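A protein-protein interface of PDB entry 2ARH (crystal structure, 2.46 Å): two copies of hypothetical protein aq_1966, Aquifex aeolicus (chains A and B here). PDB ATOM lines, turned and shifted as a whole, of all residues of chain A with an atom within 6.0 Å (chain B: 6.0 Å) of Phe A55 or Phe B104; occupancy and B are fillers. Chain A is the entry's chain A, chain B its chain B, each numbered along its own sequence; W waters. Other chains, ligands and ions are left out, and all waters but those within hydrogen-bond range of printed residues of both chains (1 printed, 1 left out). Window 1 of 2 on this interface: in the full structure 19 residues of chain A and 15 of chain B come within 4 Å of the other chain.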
ATOM      1  N   LYS A   5     -17.000   4.380 -30.439  1.00  0.00           N
ATOM      2  CA  LYS A   5     -15.736   4.538 -29.722  1.00  0.00           C
ATOM      3  C   LYS A   5     -15.428   3.360 -28.790  1.00  0.00           C
ATOM      4  O   LYS A   5     -14.340   2.760 -28.900  1.00  0.00           O
ATOM      5  CB  LYS A   5     -15.751   5.867 -28.922  1.00  0.00           C
ATOM      6  CG  LYS A   5     -14.382   6.350 -28.372  1.00  0.00           C
ATOM      7  CD  LYS A   5     -13.712   7.339 -29.398  1.00  0.00           C
ATOM      8  CE  LYS A   5     -14.098   8.801 -29.147  1.00  0.00           C
ATOM      9  NZ  LYS A   5     -14.371   8.728 -27.704  1.00  0.00           N
ATOM     10  N   PHE A  34     -19.447   7.133 -13.546  1.00  0.00           N
ATOM     11  CA  PHE A  34     -20.336   7.721 -14.539  1.00  0.00           C
ATOM     12  C   PHE A  34     -20.528   6.675 -15.603  1.00  0.00           C
ATOM     13  O   PHE A  34     -19.777   5.711 -15.641  1.00  0.00           O
ATOM     14  CB  PHE A  34     -19.804   9.074 -15.057  1.00  0.00           C
ATOM     15  CG  PHE A  34     -19.390  10.006 -13.942  1.00  0.00           C
ATOM     16  CD1 PHE A  34     -20.270  10.286 -12.890  1.00  0.00           C
ATOM     17  CD2 PHE A  34     -18.108  10.526 -13.885  1.00  0.00           C
ATOM     18  CE1 PHE A  34     -19.896  11.096 -11.850  1.00  0.00           C
ATOM     19  CE2 PHE A  34     -17.719  11.361 -12.823  1.00  0.00           C
ATOM     20  CZ  PHE A  34     -18.607  11.649 -11.837  1.00  0.00           C
ATOM     21  N   LYS A  35     -21.582   6.804 -16.398  1.00  0.00           N
ATOM     22  CA  LYS A  35     -21.994   5.732 -17.298  1.00  0.00           C
ATOM     23  C   LYS A  35     -21.014   5.426 -18.419  1.00  0.00           C
ATOM     24  O   LYS A  35     -20.857   4.265 -18.813  1.00  0.00           O
ATOM     25  CB  LYS A  35     -23.377   6.015 -17.867  1.00  0.00           C
ATOM     26  CG  LYS A  35     -23.813   5.086 -19.033  1.00  0.00           C
ATOM     27  CD  LYS A  35     -25.320   5.128 -19.163  1.00  0.00           C
ATOM     28  CE  LYS A  35     -25.721   5.390 -20.588  1.00  0.00           C
ATOM     29  NZ  LYS A  35     -25.873   6.849 -20.771  1.00  0.00           N
ATOM     30  N   GLU A  36     -20.358   6.465 -18.925  1.00  0.00           N
ATOM     31  CA  GLU A  36     -19.416   6.312 -20.062  1.00  0.00           C
ATOM     32  C   GLU A  36     -17.956   6.180 -19.616  1.00  0.00           C
ATOM     33  O   GLU A  36     -17.025   6.341 -20.441  1.00  0.00           O
ATOM     34  CB  GLU A  36     -19.562   7.471 -21.061  1.00  0.00           C
ATOM     35  CG  GLU A  36     -20.980   7.663 -21.617  1.00  0.00           C
ATOM     36  CD  GLU A  36     -21.588   6.404 -22.279  1.00  0.00           C
ATOM     37  OE1 GLU A  36     -20.853   5.526 -22.778  1.00  0.00           O
ATOM     38  OE2 GLU A  36     -22.827   6.295 -22.285  1.00  0.00           O
ATOM     39  N   GLU A  37     -17.792   5.903 -18.309  1.00  0.00           N
ATOM     40  CA  GLU A  37     -16.505   5.770 -17.652  1.00  0.00           C
ATOM     41  C   GLU A  37     -16.171   4.326 -17.272  1.00  0.00           C
ATOM     42  O   GLU A  37     -16.958   3.631 -16.659  1.00  0.00           O
ATOM     43  CB  GLU A  37     -16.448   6.684 -16.438  1.00  0.00           C
ATOM     44  CG  GLU A  37     -15.055   6.830 -15.794  1.00  0.00           C
ATOM     45  CD  GLU A  37     -15.153   7.619 -14.536  1.00  0.00           C
ATOM     46  OE1 GLU A  37     -14.664   8.750 -14.502  1.00  0.00           O
ATOM     47  OE2 GLU A  37     -15.790   7.144 -13.573  1.00  0.00           O
ATOM     48  N   PHE A  38     -14.987   3.888 -17.682  1.00  0.00           N
ATOM     49  CA  PHE A  38     -14.489   2.547 -17.419  1.00  0.00           C
ATOM     50  C   PHE A  38     -13.019   2.539 -16.980  1.00  0.00           C
ATOM     51  O   PHE A  38     -12.250   3.404 -17.368  1.00  0.00           O
ATOM     52  CB  PHE A  38     -14.655   1.703 -18.668  1.00  0.00           C
ATOM     53  CG  PHE A  38     -16.085   1.567 -19.127  1.00  0.00           C
ATOM     54  CD1 PHE A  38     -16.641   2.486 -20.030  1.00  0.00           C
ATOM     55  CD2 PHE A  38     -16.878   0.507 -18.683  1.00  0.00           C
ATOM     56  CE1 PHE A  38     -18.015   2.352 -20.481  1.00  0.00           C
ATOM     57  CE2 PHE A  38     -18.229   0.369 -19.119  1.00  0.00           C
ATOM     58  CZ  PHE A  38     -18.785   1.310 -20.016  1.00  0.00           C
ATOM     59  N   LYS A  53      -8.157   4.733 -17.478  1.00  0.00           N
ATOM     60  CA  LYS A  53      -9.499   5.206 -17.174  1.00  0.00           C
ATOM     61  C   LYS A  53     -10.033   5.959 -18.413  1.00  0.00           C
ATOM     62  O   LYS A  53      -9.506   7.012 -18.812  1.00  0.00           O
ATOM     63  CB  LYS A  53      -9.530   6.091 -15.934  1.00  0.00           C
ATOM     64  CG  LYS A  53     -10.935   6.404 -15.423  1.00  0.00           C
ATOM     65  CD  LYS A  53     -10.980   7.384 -14.292  1.00  0.00           C
ATOM     66  CE  LYS A  53     -10.397   6.814 -13.026  1.00  0.00           C
ATOM     67  NZ  LYS A  53     -11.014   5.484 -12.694  1.00  0.00           N
ATOM     68  N   VAL A  54     -11.061   5.394 -19.039  1.00  0.00           N
ATOM     69  CA  VAL A  54     -11.593   5.941 -20.281  1.00  0.00           C
ATOM     70  C   VAL A  54     -12.907   6.635 -20.002  1.00  0.00           C
ATOM     71  O   VAL A  54     -13.718   6.132 -19.213  1.00  0.00           O
ATOM     72  CB  VAL A  54     -11.784   4.846 -21.401  1.00  0.00           C
ATOM     73  CG1 VAL A  54     -10.547   3.949 -21.505  1.00  0.00           C
ATOM     74  CG2 VAL A  54     -12.964   4.018 -21.124  1.00  0.00           C
ATOM     75  N   PHE A  55     -13.092   7.817 -20.576  1.00  0.00           N
ATOM     76  CA  PHE A  55     -14.388   8.463 -20.498  1.00  0.00           C
ATOM     77  C   PHE A  55     -14.797   8.664 -21.893  1.00  0.00           C
ATOM     78  O   PHE A  55     -14.135   9.364 -22.645  1.00  0.00           O
ATOM     79  CB  PHE A  55     -14.412   9.775 -19.754  1.00  0.00           C
ATOM     80  CG  PHE A  55     -15.766  10.406 -19.719  1.00  0.00           C
ATOM     81  CD1 PHE A  55     -16.738   9.935 -18.842  1.00  0.00           C
ATOM     82  CD2 PHE A  55     -16.091  11.458 -20.579  1.00  0.00           C
ATOM     83  CE1 PHE A  55     -18.038  10.491 -18.839  1.00  0.00           C
ATOM     84  CE2 PHE A  55     -17.369  12.006 -20.568  1.00  0.00           C
ATOM     85  CZ  PHE A  55     -18.343  11.529 -19.707  1.00  0.00           C
ATOM     86  N   LEU A  56     -15.892   8.013 -22.250  1.00  0.00           N
ATOM     87  CA  LEU A  56     -16.245   7.842 -23.663  1.00  0.00           C
ATOM     88  C   LEU A  56     -16.835   9.075 -24.283  1.00  0.00           C
ATOM     89  O   LEU A  56     -16.897   9.137 -25.498  1.00  0.00           O
ATOM     90  CB  LEU A  56     -17.214   6.649 -23.849  1.00  0.00           C
ATOM     91  CG  LEU A  56     -16.645   5.271 -23.526  1.00  0.00           C
ATOM     92  CD1 LEU A  56     -17.768   4.244 -23.564  1.00  0.00           C
ATOM     93  CD2 LEU A  56     -15.588   4.922 -24.488  1.00  0.00           C
ATOM     94  N   GLY A  57     -17.315  10.018 -23.462  1.00  0.00           N
ATOM     95  CA  GLY A  57     -18.001  11.239 -23.954  1.00  0.00           C
ATOM     96  C   GLY A  57     -19.508  11.198 -23.673  1.00  0.00           C
ATOM     97  O   GLY A  57     -20.104  10.104 -23.619  1.00  0.00           O
ATOM     98  N   ARG A  58     -20.103  12.366 -23.420  1.00  0.00           N
ATOM     99  CA  ARG A  58     -21.554  12.562 -23.336  1.00  0.00           C
ATOM    100  C   ARG A  58     -21.712  13.952 -23.929  1.00  0.00           C
ATOM    101  O   ARG A  58     -21.876  14.966 -23.241  1.00  0.00           O
ATOM    102  CB  ARG A  58     -22.078  12.497 -21.889  1.00  0.00           C
ATOM    103  CG  ARG A  58     -23.615  12.476 -21.781  1.00  0.00           C
ATOM    104  CD  ARG A  58     -24.155  12.872 -20.395  1.00  0.00           C
ATOM    105  NE  ARG A  58     -25.600  13.004 -20.452  1.00  0.00           N
ATOM    106  CZ  ARG A  58     -26.434  13.327 -19.452  1.00  0.00           C
ATOM    107  NH1 ARG A  58     -25.996  13.593 -18.221  1.00  0.00           N
ATOM    108  NH2 ARG A  58     -27.769  13.379 -19.705  1.00  0.00           N
ATOM    109  N   TRP A  62     -20.050  16.594 -21.892  1.00  0.00           N
ATOM    110  CA  TRP A  62     -18.684  16.163 -21.541  1.00  0.00           C
ATOM    111  C   TRP A  62     -17.976  15.520 -22.755  1.00  0.00           C
ATOM    112  O   TRP A  62     -18.482  14.615 -23.381  1.00  0.00           O
ATOM    113  CB  TRP A  62     -18.686  15.215 -20.333  1.00  0.00           C
ATOM    114  CG  TRP A  62     -19.351  15.799 -19.073  1.00  0.00           C
ATOM    115  CD1 TRP A  62     -20.524  15.402 -18.530  1.00  0.00           C
ATOM    116  CD2 TRP A  62     -18.871  16.897 -18.234  1.00  0.00           C
ATOM    117  NE1 TRP A  62     -20.830  16.181 -17.442  1.00  0.00           N
ATOM    118  CE2 TRP A  62     -19.833  17.103 -17.237  1.00  0.00           C
ATOM    119  CE3 TRP A  62     -17.724  17.715 -18.248  1.00  0.00           C
ATOM    120  CZ2 TRP A  62     -19.684  18.092 -16.219  1.00  0.00           C
ATOM    121  CZ3 TRP A  62     -17.568  18.701 -17.252  1.00  0.00           C
ATOM    122  CH2 TRP A  62     -18.554  18.877 -16.251  1.00  0.00           C
ATOM    123  N   GLN A  63     -16.795  16.046 -23.070  1.00  0.00           N
ATOM    124  CA  GLN A  63     -15.918  15.544 -24.130  1.00  0.00           C
ATOM    125  C   GLN A  63     -15.226  14.296 -23.647  1.00  0.00           C
ATOM    126  O   GLN A  63     -14.980  14.175 -22.431  1.00  0.00           O
ATOM    127  CB  GLN A  63     -14.864  16.610 -24.463  1.00  0.00           C
ATOM    128  CG  GLN A  63     -15.459  17.895 -25.014  1.00  0.00           C
ATOM    129  CD  GLN A  63     -16.368  17.621 -26.208  1.00  0.00           C
ATOM    130  OE1 GLN A  63     -15.951  16.964 -27.175  1.00  0.00           O
ATOM    131  NE2 GLN A  63     -17.611  18.078 -26.132  1.00  0.00           N
ATOM    132  N   PRO A  64     -14.904  13.361 -24.575  1.00  0.00           N
ATOM    133  CA  PRO A  64     -14.113  12.172 -24.161  1.00  0.00           C
ATOM    134  C   PRO A  64     -12.727  12.511 -23.597  1.00  0.00           C
ATOM    135  O   PRO A  64     -12.111  13.527 -23.951  1.00  0.00           O
ATOM    136  CB  PRO A  64     -13.991  11.342 -25.452  1.00  0.00           C
ATOM    137  CG  PRO A  64     -15.069  11.879 -26.422  1.00  0.00           C
ATOM    138  CD  PRO A  64     -15.235  13.337 -26.020  1.00  0.00           C
ATOM    139  N   TRP A  65     -12.256  11.681 -22.678  1.00  0.00           N
ATOM    140  CA  TRP A  65     -10.882  11.794 -22.173  1.00  0.00           C
ATOM    141  C   TRP A  65     -10.370  10.397 -21.742  1.00  0.00           C
ATOM    142  O   TRP A  65     -11.170   9.490 -21.478  1.00  0.00           O
ATOM    143  CB  TRP A  65     -10.771  12.851 -21.054  1.00  0.00           C
ATOM    144  CG  TRP A  65     -11.702  12.626 -19.892  1.00  0.00           C
ATOM    145  CD1 TRP A  65     -12.929  13.227 -19.681  1.00  0.00           C
ATOM    146  CD2 TRP A  65     -11.511  11.700 -18.793  1.00  0.00           C
ATOM    147  NE1 TRP A  65     -13.484  12.730 -18.526  1.00  0.00           N
ATOM    148  CE2 TRP A  65     -12.629  11.811 -17.957  1.00  0.00           C
ATOM    149  CE3 TRP A  65     -10.490  10.808 -18.436  1.00  0.00           C
ATOM    150  CZ2 TRP A  65     -12.763  11.045 -16.793  1.00  0.00           C
ATOM    151  CZ3 TRP A  65     -10.609  10.093 -17.278  1.00  0.00           C
ATOM    152  CH2 TRP A  65     -11.737  10.203 -16.471  1.00  0.00           C
ATOM    153  N   VAL A  66      -9.044  10.220 -21.730  1.00  0.00           N
ATOM    154  CA  VAL A  66      -8.419   8.966 -21.265  1.00  0.00           C
ATOM    155  C   VAL A  66      -7.331   9.349 -20.284  1.00  0.00           C
ATOM    156  O   VAL A  66      -6.602  10.320 -20.469  1.00  0.00           O
ATOM    157  CB  VAL A  66      -7.914   8.072 -22.433  1.00  0.00           C
ATOM    158  CG1 VAL A  66      -6.768   8.744 -23.245  1.00  0.00           C
ATOM    159  CG2 VAL A  66      -7.507   6.654 -21.962  1.00  0.00           C
ATOM    160  N   PHE A  96      -9.098  10.104 -28.465  1.00  0.00           N
ATOM    161  CA  PHE A  96      -9.354  11.078 -27.387  1.00  0.00           C
ATOM    162  C   PHE A  96      -8.704  12.435 -27.625  1.00  0.00           C
ATOM    163  O   PHE A  96      -7.519  12.495 -27.845  1.00  0.00           O
ATOM    164  CB  PHE A  96      -8.913  10.534 -26.030  1.00  0.00           C
ATOM    165  CG  PHE A  96      -9.595   9.268 -25.645  1.00  0.00           C
ATOM    166  CD1 PHE A  96      -8.989   8.020 -25.902  1.00  0.00           C
ATOM    167  CD2 PHE A  96     -10.821   9.302 -24.976  1.00  0.00           C
ATOM    168  CE1 PHE A  96      -9.637   6.805 -25.535  1.00  0.00           C
ATOM    169  CE2 PHE A  96     -11.482   8.094 -24.600  1.00  0.00           C
ATOM    170  CZ  PHE A  96     -10.887   6.855 -24.889  1.00  0.00           C
ATOM    171  N   GLU B 102     -22.903  16.875  -6.281  1.00  0.00           N
ATOM    172  CA  GLU B 102     -22.274  16.535  -7.535  1.00  0.00           C
ATOM    173  C   GLU B 102     -23.233  16.761  -8.731  1.00  0.00           C
ATOM    174  O   GLU B 102     -24.351  16.232  -8.735  1.00  0.00           O
ATOM    175  CB  GLU B 102     -21.731  15.104  -7.470  1.00  0.00           C
ATOM    176  CG  GLU B 102     -20.827  14.697  -8.654  1.00  0.00           C
ATOM    177  CD  GLU B 102     -20.308  13.272  -8.511  1.00  0.00           C
ATOM    178  OE1 GLU B 102     -19.072  13.108  -8.455  1.00  0.00           O
ATOM    179  OE2 GLU B 102     -21.127  12.323  -8.398  1.00  0.00           O
ATOM    180  N   TYR B 103     -22.817  17.561  -9.724  1.00  0.00           N
ATOM    181  CA  TYR B 103     -23.715  17.877 -10.848  1.00  0.00           C
ATOM    182  C   TYR B 103     -23.403  17.172 -12.173  1.00  0.00           C
ATOM    183  O   TYR B 103     -24.060  17.451 -13.168  1.00  0.00           O
ATOM    184  CB  TYR B 103     -23.827  19.390 -11.093  1.00  0.00           C
ATOM    185  CG  TYR B 103     -22.514  20.049 -11.449  1.00  0.00           C
ATOM    186  CD1 TYR B 103     -21.763  20.701 -10.475  1.00  0.00           C
ATOM    187  CD2 TYR B 103     -22.015  20.015 -12.764  1.00  0.00           C
ATOM    188  CE1 TYR B 103     -20.562  21.296 -10.783  1.00  0.00           C
ATOM    189  CE2 TYR B 103     -20.836  20.598 -13.085  1.00  0.00           C
ATOM    190  CZ  TYR B 103     -20.101  21.245 -12.079  1.00  0.00           C
ATOM    191  OH  TYR B 103     -18.892  21.852 -12.370  1.00  0.00           O
ATOM    192  N   PHE B 104     -22.428  16.268 -12.165  1.00  0.00           N
ATOM    193  CA  PHE B 104     -21.855  15.684 -13.340  1.00  0.00           C
ATOM    194  C   PHE B 104     -22.916  14.977 -14.173  1.00  0.00           C
ATOM    195  O   PHE B 104     -22.932  15.072 -15.397  1.00  0.00           O
ATOM    196  CB  PHE B 104     -20.714  14.720 -12.945  1.00  0.00           C
ATOM    197  CG  PHE B 104     -19.853  14.267 -14.128  1.00  0.00           C
ATOM    198  CD1 PHE B 104     -18.603  14.839 -14.347  1.00  0.00           C
ATOM    199  CD2 PHE B 104     -20.326  13.292 -15.052  1.00  0.00           C
ATOM    200  CE1 PHE B 104     -17.797  14.457 -15.435  1.00  0.00           C
ATOM    201  CE2 PHE B 104     -19.530  12.876 -16.133  1.00  0.00           C
ATOM    202  CZ  PHE B 104     -18.250  13.455 -16.311  1.00  0.00           C
ATOM    203  N   GLU B 105     -23.828  14.294 -13.495  1.00  0.00           N
ATOM    204  CA  GLU B 105     -24.899  13.551 -14.179  1.00  0.00           C
ATOM    205  C   GLU B 105     -26.045  14.433 -14.614  1.00  0.00           C
ATOM    206  O   GLU B 105     -26.855  13.999 -15.407  1.00  0.00           O
ATOM    207  CB  GLU B 105     -25.408  12.396 -13.298  1.00  0.00           C
ATOM    208  CG  GLU B 105     -24.446  11.205 -13.148  1.00  0.00           C
ATOM    209  CD  GLU B 105     -24.098  10.583 -14.493  1.00  0.00           C
ATOM    210  OE1 GLU B 105     -24.994  10.392 -15.352  1.00  0.00           O
ATOM    211  OE2 GLU B 105     -22.932  10.297 -14.719  1.00  0.00           O
ATOM    212  N   ASP B 106     -26.096  15.678 -14.111  1.00  0.00           N
ATOM    213  CA  ASP B 106     -27.147  16.664 -14.428  1.00  0.00           C
ATOM    214  C   ASP B 106     -26.738  17.558 -15.626  1.00  0.00           C
ATOM    215  O   ASP B 106     -25.874  18.475 -15.487  1.00  0.00           O
ATOM    216  CB  ASP B 106     -27.384  17.506 -13.187  1.00  0.00           C
ATOM    217  CG  ASP B 106     -28.507  18.465 -13.341  1.00  0.00           C
ATOM    218  OD1 ASP B 106     -28.794  19.208 -12.371  1.00  0.00           O
ATOM    219  OD2 ASP B 106     -29.146  18.480 -14.400  1.00  0.00           O
ATOM    220  N   LYS B 107     -27.331  17.281 -16.795  1.00  0.00           N
ATOM    221  CA  LYS B 107     -26.831  17.829 -18.067  1.00  0.00           C
ATOM    222  C   LYS B 107     -27.200  19.297 -18.234  1.00  0.00           C
ATOM    223  O   LYS B 107     -26.420  20.082 -18.781  1.00  0.00           O
ATOM    224  CB  LYS B 107     -27.331  17.017 -19.280  1.00  0.00           C
ATOM    225  CG  LYS B 107     -28.918  16.971 -19.359  1.00  0.00           C
ATOM    226  CD  LYS B 107     -29.456  16.185 -20.488  1.00  0.00           C
ATOM    227  CE  LYS B 107     -31.002  16.135 -20.396  1.00  0.00           C
ATOM    228  NZ  LYS B 107     -31.633  15.521 -21.621  1.00  0.00           N
ATOM    229  N   THR B 110     -24.968  21.281 -15.905  1.00  0.00           N
ATOM    230  CA  THR B 110     -23.670  21.179 -16.569  1.00  0.00           C
ATOM    231  C   THR B 110     -23.551  22.194 -17.698  1.00  0.00           C
ATOM    232  O   THR B 110     -22.707  23.093 -17.665  1.00  0.00           O
ATOM    233  CB  THR B 110     -23.419  19.713 -17.029  1.00  0.00           C
ATOM    234  OG1 THR B 110     -23.187  18.932 -15.863  1.00  0.00           O
ATOM    235  CG2 THR B 110     -22.200  19.565 -17.967  1.00  0.00           C
ATOM    236  N   GLU B 143     -11.971  15.317 -13.850  1.00  0.00           N
ATOM    237  CA  GLU B 143     -11.908  13.906 -13.456  1.00  0.00           C
ATOM    238  C   GLU B 143     -10.707  13.526 -14.345  1.00  0.00           C
ATOM    239  O   GLU B 143     -10.481  14.150 -15.391  1.00  0.00           O
ATOM    240  CB  GLU B 143     -13.156  13.130 -13.879  1.00  0.00           C
ATOM    241  CG  GLU B 143     -14.492  13.801 -13.667  1.00  0.00           C
ATOM    242  CD  GLU B 143     -15.067  13.681 -12.254  1.00  0.00           C
ATOM    243  OE1 GLU B 143     -14.690  12.761 -11.469  1.00  0.00           O
ATOM    244  OE2 GLU B 143     -15.916  14.542 -11.933  1.00  0.00           O
ATOM    245  N   HIS B 150     -16.661  17.788  -9.696  1.00  0.00           N
ATOM    246  CA  HIS B 150     -17.753  18.597 -10.330  1.00  0.00           C
ATOM    247  C   HIS B 150     -18.966  18.712  -9.411  1.00  0.00           C
ATOM    248  O   HIS B 150     -19.974  18.005  -9.577  1.00  0.00           O
ATOM    249  CB  HIS B 150     -18.151  18.046 -11.719  1.00  0.00           C
ATOM    250  CG  HIS B 150     -17.018  18.079 -12.692  1.00  0.00           C
ATOM    251  ND1 HIS B 150     -16.646  19.234 -13.358  1.00  0.00           N
ATOM    252  CD2 HIS B 150     -16.088  17.146 -13.000  1.00  0.00           C
ATOM    253  CE1 HIS B 150     -15.567  18.983 -14.079  1.00  0.00           C
ATOM    254  NE2 HIS B 150     -15.208  17.725 -13.876  1.00  0.00           N
HETATM  255  O   HOH W   1     -28.774  14.442 -17.045  1.00  0.00           O
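Glu A36 touches none of the printed residues of chain B.
Of the printed residues of chain B, Trp A62 touches Phe B104 (3.1 Å), Thr B110 (3.4 Å) and His B150 (3.5 Å).
Of the printed residues of chain B, Trp A65 touches Glu B143.
Of the printed residues of chain A, Glu B102 touches Phe A34.
Phe B104 touches three residues of chain A.
Of the printed residues of chain A, Glu B105 touches Phe A34 and Arg A58.
Of the printed residues of chain A, Thr B110 touches Trp A62.
Printed residues of chain A that touch a printed residue of chain B: Phe A34, Phe A55, Arg A58, Trp A62 and Trp A65.
Of the 9 printed residues of chain B, 7 touch a printed residue of chain A.
Printed residues of chain B that touch a printed residue of chain A: Glu B102, Phe B104, Glu B105, Lys B107, Thr B110, Glu B143 and His B150.
Hydrophobic or aromatic side chains of chain B that line the printed part of chain A: Phe B104 and His B150.
CZ of Phe A34 touches OE1 of Glu B102, 3.7 Å away.
Phe A34 touches Phe B104 (CD2 to CE2, 3.5 Å).
Phe A34 touches Glu B105 (CD1 to OE2, 3.2 Å).
CE2 of Phe A34 touches CD of Glu B143, 3.6 Å away.
CE1 of Phe A55 touches CZ of Phe B104 (3.9 Å).
Lys B107 touches Arg A58.
Trp A62 touches Thr B110 (CZ2 to CG2, 3.4 Å).
ND1 of His B150 touches CH2 of Trp A62, 3.5 Å away.
Trp A65 touches Glu B143 (CZ2 to CB, 3.6 Å).
O of Asp B106 is in hydrogen-bond range of OG1 of Thr B110.
O of His B150 sits at hydrogen-bond distance from N of Tyr B103, at 2.9 Å.
N of Phe A55 lies within hydrogen-bond range of O of Trp A65, at 2.7 Å.
The side-chain hydroxyl (OG1) of Thr B110 lies within hydrogen-bond range of the backbone carbonyl oxygen (O) of Tyr B103, 3.2 Å away.
No position is printed for both chains.
Of the 11 pairs that touch across the chains among the printed residues, none has its exchanged pair printed and touching as well.
Water W1 lies within hydrogen-bond range of the backbone carbonyl oxygen of Glu B105, the guanidinium group of Arg A58 and the backbone NH of Lys B107.
The guanidinium group (NH1) of Arg A58 lies within hydrogen-bond range of the backbone carbonyl oxygen (O) of Glu B105, at 3.0 Å.
The indole nitrogen (NE1) of Trp A62 sits at hydrogen-bond distance from the backbone carbonyl oxygen (O) of Phe B104, 3.1 Å away.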
